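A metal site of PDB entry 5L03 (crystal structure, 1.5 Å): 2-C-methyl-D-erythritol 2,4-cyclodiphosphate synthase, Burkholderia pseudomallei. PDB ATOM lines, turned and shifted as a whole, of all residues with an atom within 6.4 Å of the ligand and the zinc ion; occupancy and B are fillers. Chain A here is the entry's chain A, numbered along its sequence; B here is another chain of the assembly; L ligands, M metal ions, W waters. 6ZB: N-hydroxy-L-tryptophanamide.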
ATOM      1  N   ASP A  10     -24.920 -24.745  18.454  1.00  0.00           N
ATOM      2  CA  ASP A  10     -25.008 -24.284  19.834  1.00  0.00           C
ATOM      3  C   ASP A  10     -24.253 -22.967  19.970  1.00  0.00           C
ATOM      4  O   ASP A  10     -23.354 -22.650  19.195  1.00  0.00           O
ATOM      5  CB  ASP A  10     -24.513 -25.364  20.799  1.00  0.00           C
ATOM      6  CG  ASP A  10     -24.878 -25.088  22.261  1.00  0.00           C
ATOM      7  OD1 ASP A  10     -25.906 -24.407  22.513  1.00  0.00           O
ATOM      8  OD2 ASP A  10     -24.202 -25.631  23.156  1.00  0.00           O
ATOM      9  N   VAL A  11     -24.649 -22.205  20.982  1.00  0.00           N
ATOM     10  CA  VAL A  11     -23.973 -20.965  21.320  1.00  0.00           C
ATOM     11  C   VAL A  11     -24.087 -20.792  22.830  1.00  0.00           C
ATOM     12  O   VAL A  11     -25.097 -21.152  23.434  1.00  0.00           O
ATOM     13  CB  VAL A  11     -24.552 -19.749  20.547  1.00  0.00           C
ATOM     14  CG1 VAL A  11     -25.969 -19.423  21.013  1.00  0.00           C
ATOM     15  CG2 VAL A  11     -23.610 -18.539  20.663  1.00  0.00           C
ATOM     16  N   HIS A  12     -23.024 -20.248  23.433  1.00  0.00           N
ATOM     17  CA  HIS A  12     -23.062 -19.885  24.843  1.00  0.00           C
ATOM     18  C   HIS A  12     -22.353 -18.563  25.038  1.00  0.00           C
ATOM     19  O   HIS A  12     -21.409 -18.239  24.310  1.00  0.00           O
ATOM     20  CB  HIS A  12     -22.322 -20.920  25.722  1.00  0.00           C
ATOM     21  CG  HIS A  12     -23.068 -22.205  25.898  1.00  0.00           C
ATOM     22  ND1 HIS A  12     -23.882 -22.452  26.991  1.00  0.00           N
ATOM     23  CD2 HIS A  12     -23.126 -23.315  25.136  1.00  0.00           C
ATOM     24  CE1 HIS A  12     -24.411 -23.648  26.878  1.00  0.00           C
ATOM     25  NE2 HIS A  12     -23.962 -24.201  25.770  1.00  0.00           N
ATOM     26  N   LEU A  34     -21.012 -19.948  29.812  1.00  0.00           N
ATOM     27  CA  LEU A  34     -22.055 -19.933  30.838  1.00  0.00           C
ATOM     28  C   LEU A  34     -23.141 -20.939  30.466  1.00  0.00           C
ATOM     29  O   LEU A  34     -23.688 -20.884  29.354  1.00  0.00           O
ATOM     30  CB  LEU A  34     -22.671 -18.533  30.921  1.00  0.00           C
ATOM     31  CG  LEU A  34     -23.871 -18.414  31.856  1.00  0.00           C
ATOM     32  CD1 LEU A  34     -23.457 -18.832  33.263  1.00  0.00           C
ATOM     33  CD2 LEU A  34     -24.390 -16.987  31.827  1.00  0.00           C
ATOM     34  N   GLY A  35     -23.445 -21.832  31.392  1.00  0.00           N
ATOM     35  CA  GLY A  35     -24.522 -22.785  31.175  1.00  0.00           C
ATOM     36  C   GLY A  35     -24.806 -23.521  32.459  1.00  0.00           C
ATOM     37  O   GLY A  35     -24.093 -23.369  33.457  1.00  0.00           O
ATOM     38  N   HIS A  36     -25.891 -24.301  32.440  1.00  0.00           N
ATOM     39  CA  HIS A  36     -26.183 -25.183  33.565  1.00  0.00           C
ATOM     40  C   HIS A  36     -25.162 -26.303  33.657  1.00  0.00           C
ATOM     41  O   HIS A  36     -24.597 -26.564  34.730  1.00  0.00           O
ATOM     42  CB  HIS A  36     -27.597 -25.752  33.422  1.00  0.00           C
ATOM     43  CG  HIS A  36     -27.999 -26.705  34.512  1.00  0.00           C
ATOM     44  ND1 HIS A  36     -28.233 -26.308  35.810  1.00  0.00           N
ATOM     45  CD2 HIS A  36     -28.214 -28.051  34.484  1.00  0.00           C
ATOM     46  CE1 HIS A  36     -28.581 -27.359  36.539  1.00  0.00           C
ATOM     47  NE2 HIS A  36     -28.572 -28.426  35.760  1.00  0.00           N
ATOM     48  N   SER A  37     -24.900 -26.966  32.536  1.00  0.00           N
ATOM     49  CA  SER A  37     -23.818 -27.947  32.429  1.00  0.00           C
ATOM     50  C   SER A  37     -22.479 -27.218  32.396  1.00  0.00           C
ATOM     51  O   SER A  37     -22.370 -26.021  32.683  1.00  0.00           O
ATOM     52  CB  SER A  37     -24.000 -28.763  31.167  1.00  0.00           C
ATOM     53  OG  SER A  37     -23.733 -27.973  30.000  1.00  0.00           O
ATOM     54  N   ASP A  38     -21.424 -27.947  32.005  1.00  0.00           N
ATOM     55  CA  ASP A  38     -20.141 -27.285  31.777  1.00  0.00           C
ATOM     56  C   ASP A  38     -20.135 -26.379  30.546  1.00  0.00           C
ATOM     57  O   ASP A  38     -19.118 -25.731  30.258  1.00  0.00           O
ATOM     58  CB  ASP A  38     -18.988 -28.305  31.728  1.00  0.00           C
ATOM     59  CG  ASP A  38     -19.038 -29.251  30.533  1.00  0.00           C
ATOM     60  OD1 ASP A  38     -19.831 -29.033  29.576  1.00  0.00           O
ATOM     61  OD2 ASP A  38     -18.239 -30.225  30.534  1.00  0.00           O
ATOM     62  N   ALA A  39     -21.240 -26.329  29.808  1.00  0.00           N
ATOM     63  CA  ALA A  39     -21.443 -25.385  28.712  1.00  0.00           C
ATOM     64  C   ALA A  39     -20.509 -25.635  27.530  1.00  0.00           C
ATOM     65  O   ALA A  39     -20.177 -24.692  26.797  1.00  0.00           O
ATOM     66  CB  ALA A  39     -21.353 -23.916  29.178  1.00  0.00           C
ATOM     67  N   ASP A  40     -20.130 -26.892  27.298  1.00  0.00           N
ATOM     68  CA  ASP A  40     -19.250 -27.245  26.186  1.00  0.00           C
ATOM     69  C   ASP A  40     -19.995 -27.141  24.855  1.00  0.00           C
ATOM     70  O   ASP A  40     -20.648 -28.077  24.399  1.00  0.00           O
ATOM     71  CB  ASP A  40     -18.678 -28.650  26.384  1.00  0.00           C
ATOM     72  CG  ASP A  40     -17.510 -28.929  25.466  1.00  0.00           C
ATOM     73  OD1 ASP A  40     -17.532 -28.488  24.287  1.00  0.00           O
ATOM     74  OD2 ASP A  40     -16.599 -29.652  25.908  1.00  0.00           O
ATOM     75  N   VAL A  41     -19.862 -25.981  24.229  1.00  0.00           N
ATOM     76  CA  VAL A  41     -20.662 -25.633  23.052  1.00  0.00           C
ATOM     77  C   VAL A  41     -20.400 -26.597  21.901  1.00  0.00           C
ATOM     78  O   VAL A  41     -21.311 -26.939  21.127  1.00  0.00           O
ATOM     79  CB  VAL A  41     -20.399 -24.158  22.696  1.00  0.00           C
ATOM     80  CG1 VAL A  41     -18.960 -23.932  22.230  1.00  0.00           C
ATOM     81  CG2 VAL A  41     -21.366 -23.682  21.626  1.00  0.00           C
ATOM     82  N   HIS A  44     -22.030 -30.020  22.617  1.00  0.00           N
ATOM     83  CA  HIS A  44     -23.488 -29.930  22.506  1.00  0.00           C
ATOM     84  C   HIS A  44     -23.941 -29.903  21.056  1.00  0.00           C
ATOM     85  O   HIS A  44     -24.930 -30.568  20.707  1.00  0.00           O
ATOM     86  CB  HIS A  44     -24.028 -28.708  23.237  1.00  0.00           C
ATOM     87  CG  HIS A  44     -23.789 -28.730  24.696  1.00  0.00           C
ATOM     88  ND1 HIS A  44     -23.977 -27.640  25.514  1.00  0.00           N
ATOM     89  CD2 HIS A  44     -23.261 -29.710  25.482  1.00  0.00           C
ATOM     90  CE1 HIS A  44     -23.631 -27.954  26.747  1.00  0.00           C
ATOM     91  NE2 HIS A  44     -23.184 -29.198  26.755  1.00  0.00           N
ATOM     92  N   ALA A  45     -23.240 -29.152  20.194  1.00  0.00           N
ATOM     93  CA  ALA A  45     -23.624 -29.143  18.793  1.00  0.00           C
ATOM     94  C   ALA A  45     -23.479 -30.521  18.175  1.00  0.00           C
ATOM     95  O   ALA A  45     -24.338 -30.957  17.395  1.00  0.00           O
ATOM     96  CB  ALA A  45     -22.750 -28.145  18.030  1.00  0.00           C
ATOM     97  N   ILE A  59     -30.971 -32.373  22.246  1.00  0.00           N
ATOM     98  CA  ILE A  59     -30.232 -32.525  23.494  1.00  0.00           C
ATOM     99  C   ILE A  59     -31.087 -32.108  24.691  1.00  0.00           C
ATOM    100  O   ILE A  59     -31.032 -32.736  25.767  1.00  0.00           O
ATOM    101  CB  ILE A  59     -28.895 -31.749  23.408  1.00  0.00           C
ATOM    102  CG1 ILE A  59     -28.017 -32.094  24.613  1.00  0.00           C
ATOM    103  CG2 ILE A  59     -29.153 -30.237  23.179  1.00  0.00           C
ATOM    104  CD1 ILE A  59     -26.597 -31.500  24.536  1.00  0.00           C
ATOM    105  N   GLY A  60     -31.936 -31.092  24.512  1.00  0.00           N
ATOM    106  CA  GLY A  60     -32.805 -30.640  25.593  1.00  0.00           C
ATOM    107  C   GLY A  60     -33.854 -31.665  25.971  1.00  0.00           C
ATOM    108  O   GLY A  60     -34.227 -31.769  27.142  1.00  0.00           O
ATOM    109  N   ARG A  61     -34.338 -32.445  24.992  1.00  0.00           N
ATOM    110  CA  ARG A  61     -35.285 -33.506  25.296  1.00  0.00           C
ATOM    111  C   ARG A  61     -34.622 -34.610  26.101  1.00  0.00           C
ATOM    112  O   ARG A  61     -35.238 -35.178  27.005  1.00  0.00           O
ATOM    113  CB  ARG A  61     -35.803 -34.108  23.980  1.00  0.00           C
ATOM    114  CG  ARG A  61     -36.520 -35.441  24.125  1.00  0.00           C
ATOM    115  CD  ARG A  61     -36.971 -35.973  22.762  1.00  0.00           C
ATOM    116  NE  ARG A  61     -37.010 -37.421  22.719  1.00  0.00           N
ATOM    117  CZ  ARG A  61     -37.448 -38.134  21.692  1.00  0.00           C
ATOM    118  NH1 ARG A  61     -37.914 -37.520  20.599  1.00  0.00           N
ATOM    119  NH2 ARG A  61     -37.428 -39.462  21.742  1.00  0.00           N
ATOM    120  N   PHE A  63     -31.596 -34.517  28.027  1.00  0.00           N
ATOM    121  CA  PHE A  63     -30.953 -34.159  29.295  1.00  0.00           C
ATOM    122  C   PHE A  63     -31.590 -32.863  29.757  1.00  0.00           C
ATOM    123  O   PHE A  63     -31.542 -31.853  29.052  1.00  0.00           O
ATOM    124  CB  PHE A  63     -29.449 -33.976  29.072  1.00  0.00           C
ATOM    125  CG  PHE A  63     -28.776 -35.132  28.344  1.00  0.00           C
ATOM    126  CD1 PHE A  63     -28.670 -36.387  28.918  1.00  0.00           C
ATOM    127  CD2 PHE A  63     -28.224 -34.940  27.086  1.00  0.00           C
ATOM    128  CE1 PHE A  63     -28.057 -37.426  28.243  1.00  0.00           C
ATOM    129  CE2 PHE A  63     -27.589 -35.984  26.407  1.00  0.00           C
ATOM    130  CZ  PHE A  63     -27.518 -37.221  26.998  1.00  0.00           C
ATOM    131  N   SER A  64     -32.188 -32.886  30.954  1.00  0.00           N
ATOM    132  CA  SER A  64     -32.904 -31.718  31.464  1.00  0.00           C
ATOM    133  C   SER A  64     -31.926 -30.655  31.958  1.00  0.00           C
ATOM    134  O   SER A  64     -31.135 -30.918  32.874  1.00  0.00           O
ATOM    135  CB  SER A  64     -33.842 -32.127  32.588  1.00  0.00           C
ATOM    136  OG  SER A  64     -34.336 -30.975  33.240  1.00  0.00           O
ATOM    137  N   ASP A  65     -32.028 -29.448  31.408  1.00  0.00           N
ATOM    138  CA  ASP A  65     -31.147 -28.352  31.800  1.00  0.00           C
ATOM    139  C   ASP A  65     -31.527 -27.706  33.138  1.00  0.00           C
ATOM    140  O   ASP A  65     -30.947 -26.684  33.497  1.00  0.00           O
ATOM    141  CB  ASP A  65     -31.040 -27.292  30.692  1.00  0.00           C
ATOM    142  CG  ASP A  65     -32.380 -26.628  30.383  1.00  0.00           C
ATOM    143  OD1 ASP A  65     -33.388 -26.897  31.069  1.00  0.00           O
ATOM    144  OD2 ASP A  65     -32.397 -25.810  29.424  1.00  0.00           O
ATOM    145  N   THR A  66     -32.491 -28.276  33.861  1.00  0.00           N
ATOM    146  CA  THR A  66     -32.816 -27.837  35.212  1.00  0.00           C
ATOM    147  C   THR A  66     -32.668 -28.948  36.253  1.00  0.00           C
ATOM    148  O   THR A  66     -32.865 -28.694  37.447  1.00  0.00           O
ATOM    149  CB  THR A  66     -34.231 -27.240  35.276  1.00  0.00           C
ATOM    150  OG1 THR A  66     -35.179 -28.167  34.715  1.00  0.00           O
ATOM    151  CG2 THR A  66     -34.287 -25.925  34.512  1.00  0.00           C
ATOM    152  N   PHE A  70     -27.424 -32.499  36.520  1.00  0.00           N
ATOM    153  CA  PHE A  70     -26.658 -32.004  35.383  1.00  0.00           C
ATOM    154  C   PHE A  70     -25.989 -30.661  35.653  1.00  0.00           C
ATOM    155  O   PHE A  70     -25.372 -30.094  34.734  1.00  0.00           O
ATOM    156  CB  PHE A  70     -27.543 -31.891  34.130  1.00  0.00           C
ATOM    157  CG  PHE A  70     -28.031 -33.211  33.607  1.00  0.00           C
ATOM    158  CD1 PHE A  70     -27.154 -34.271  33.420  1.00  0.00           C
ATOM    159  CD2 PHE A  70     -29.378 -33.401  33.319  1.00  0.00           C
ATOM    160  CE1 PHE A  70     -27.608 -35.484  32.938  1.00  0.00           C
ATOM    161  CE2 PHE A  70     -29.832 -34.615  32.837  1.00  0.00           C
ATOM    162  CZ  PHE A  70     -28.957 -35.661  32.649  1.00  0.00           C
ATOM    163  N   ALA A  73     -22.462 -30.570  34.648  1.00  0.00           N
ATOM    164  CA  ALA A  73     -22.286 -31.879  34.036  1.00  0.00           C
ATOM    165  C   ALA A  73     -21.145 -31.889  33.027  1.00  0.00           C
ATOM    166  O   ALA A  73     -20.962 -30.938  32.251  1.00  0.00           O
ATOM    167  CB  ALA A  73     -23.577 -32.313  33.337  1.00  0.00           C
ATOM    168  N   SER A  75     -19.839 -32.669  29.748  1.00  0.00           N
ATOM    169  CA  SER A  75     -20.512 -32.860  28.471  1.00  0.00           C
ATOM    170  C   SER A  75     -19.933 -34.010  27.656  1.00  0.00           C
ATOM    171  O   SER A  75     -20.582 -34.459  26.697  1.00  0.00           O
ATOM    172  CB  SER A  75     -20.612 -31.566  27.661  1.00  0.00           C
ATOM    173  OG  SER A  75     -21.409 -30.599  28.343  1.00  0.00           O
ATOM    174  N   LEU A  78     -22.192 -36.710  28.638  1.00  0.00           N
ATOM    175  CA  LEU A  78     -23.452 -36.558  27.904  1.00  0.00           C
ATOM    176  C   LEU A  78     -23.298 -37.015  26.459  1.00  0.00           C
ATOM    177  O   LEU A  78     -24.190 -37.671  25.912  1.00  0.00           O
ATOM    178  CB  LEU A  78     -23.919 -35.106  27.949  1.00  0.00           C
ATOM    179  CG  LEU A  78     -24.199 -34.581  29.351  1.00  0.00           C
ATOM    180  CD1 LEU A  78     -24.779 -33.173  29.238  1.00  0.00           C
ATOM    181  CD2 LEU A  78     -25.133 -35.508  30.127  1.00  0.00           C
ATOM    182  N   LYS B 134     -33.886 -24.595  19.895  1.00  0.00           N
ATOM    183  CA  LYS B 134     -32.818 -23.936  20.628  1.00  0.00           C
ATOM    184  C   LYS B 134     -33.225 -22.501  20.914  1.00  0.00           C
ATOM    185  O   LYS B 134     -33.930 -21.878  20.119  1.00  0.00           O
ATOM    186  CB  LYS B 134     -31.562 -23.811  19.737  1.00  0.00           C
ATOM    187  CG  LYS B 134     -30.856 -25.106  19.409  1.00  0.00           C
ATOM    188  CD  LYS B 134     -30.064 -25.504  20.623  1.00  0.00           C
ATOM    189  CE  LYS B 134     -28.981 -24.456  20.857  1.00  0.00           C
ATOM    190  NZ  LYS B 134     -28.557 -24.387  22.273  1.00  0.00           N
ATOM    191  N   GLU B 137     -29.431 -18.022  23.668  1.00  0.00           N
ATOM    192  CA  GLU B 137     -28.764 -17.591  24.906  1.00  0.00           C
ATOM    193  C   GLU B 137     -28.668 -16.070  25.001  1.00  0.00           C
ATOM    194  O   GLU B 137     -27.663 -15.519  25.448  1.00  0.00           O
ATOM    195  CB  GLU B 137     -27.376 -18.247  25.006  1.00  0.00           C
ATOM    196  CG  GLU B 137     -27.410 -19.758  25.229  1.00  0.00           C
ATOM    197  CD  GLU B 137     -27.905 -20.166  26.600  1.00  0.00           C
ATOM    198  OE1 GLU B 137     -28.529 -21.240  26.708  1.00  0.00           O
ATOM    199  OE2 GLU B 137     -27.700 -19.399  27.561  1.00  0.00           O
HETATM  200  O   6ZB L   1     -28.009 -26.163  28.333  1.00  0.00           O
HETATM  201  C   6ZB L   1     -27.256 -26.265  27.384  1.00  0.00           C
HETATM  202  N03 6ZB L   1     -25.817 -26.189  27.713  1.00  0.00           N
HETATM  203  O04 6ZB L   1     -25.492 -25.995  29.029  1.00  0.00           O
HETATM  204  CA  6ZB L   1     -27.752 -26.504  25.883  1.00  0.00           C
HETATM  205  N   6ZB L   1     -26.753 -25.965  25.037  1.00  0.00           N
HETATM  206  CB  6ZB L   1     -27.952 -27.994  25.671  1.00  0.00           C
HETATM  207  CG  6ZB L   1     -28.602 -28.676  26.783  1.00  0.00           C
HETATM  208  CD2 6ZB L   1     -27.977 -29.349  27.872  1.00  0.00           C
HETATM  209  CE2 6ZB L   1     -29.041 -29.846  28.717  1.00  0.00           C
HETATM  210  NE1 6ZB L   1     -30.283 -29.481  28.174  1.00  0.00           N
HETATM  211  CD1 6ZB L   1     -29.985 -28.786  27.015  1.00  0.00           C
HETATM  212  CE3 6ZB L   1     -26.664 -29.600  28.246  1.00  0.00           C
HETATM  213  CZ3 6ZB L   1     -26.403 -30.314  29.402  1.00  0.00           C
HETATM  214  CH2 6ZB L   1     -27.435 -30.808  30.222  1.00  0.00           C
HETATM  215  CZ2 6ZB L   1     -28.751 -30.569  29.890  1.00  0.00           C
HETATM  216 ZN    ZN M   1     -24.841 -25.886  25.034  1.00  0.00          ZN
HETATM  217  O   HOH W   1     -30.341 -25.063  28.106  1.00  0.00           O
HETATM  218  O   HOH W   2     -30.586 -27.182  23.651  1.00  0.00           O
HETATM  219  O   HOH W   3     -33.284 -29.440  29.002  1.00  0.00           O
HETATM  220  O   HOH W   4     -27.163 -22.988  24.683  1.00  0.00           O
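The zinc ion is bound by N of the ligand (1.9 Å), OD2 of Asp 10 (2.0 Å), ND1 of His 44 (2.0 Å) and NE2 of His 12 (2.0 Å). The zinc ion has four donor atoms within binding distance.
OG of Ser 37 sits at hydrogen-bond distance from O04 of the ligand (2.8 Å). NE1 of the ligand sits at hydrogen-bond distance from O of Phe 63 (2.8 Å).
Within 4 Å of the zinc ion: Asp 10, His 12 and His 44. The nearest printed residue that does not touch the zinc ion is Val 41 (4.6 Å).
Residues that only touch the ligand: Gly 35, His 36, Ile 59, Gly 60, Ser 64, Asp 65, Leu 78 and Lys 134 of chain B. Hydrophobic or aromatic side chains that line the ligand: His 12, His 44, Ile 59, Phe 63 and Leu 78. Within 4 Å of the ligand: Asp 10, His 12, Gly 35, His 36, Ser 37, His 44, Ile 59, Gly 60, Phe 63, Ser 64, Asp 65, Leu 78 and Lys 134 of chain B.
A ring nitrogen (NE2) of His 44 lies within hydrogen-bond range of the side-chain hydroxyl (OG) of Ser 75 (2.8 Å). A ring nitrogen (ND1) of His 12 lies within hydrogen-bond range of the backbone carbonyl oxygen of Leu 34, 2.8 Å away. The side-chain carboxylate (OD1) of Asp 10 is in salt-bridge range of the side-chain amino group (NZ) of Lys 134 of chain B (2.7 Å). The side-chain hydroxyl (OG) of Ser 37 sits at hydrogen-bond distance from the backbone NH (N) of Ala 39, at 3.0 Å. The side-chain hydroxyl (OG1) of Thr 66 lies within hydrogen-bond range of the side-chain hydroxyl (OG) of Ser 64, at 3.3 Å.
Water W1 bridges the side-chain carboxylate (OD2) of Asp 65 (2.6 Å) and an oxygen (O) of the ligand (2.6 Å). Water W3 lies within hydrogen-bond range of the backbone NH of Asp 65 (2.7 Å), the backbone carbonyl oxygen of Phe 63 (3.0 Å), a nitrogen (NE1) of the ligand (3.1 Å) and the backbone carbonyl oxygen of Gly 60 (3.1 Å).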
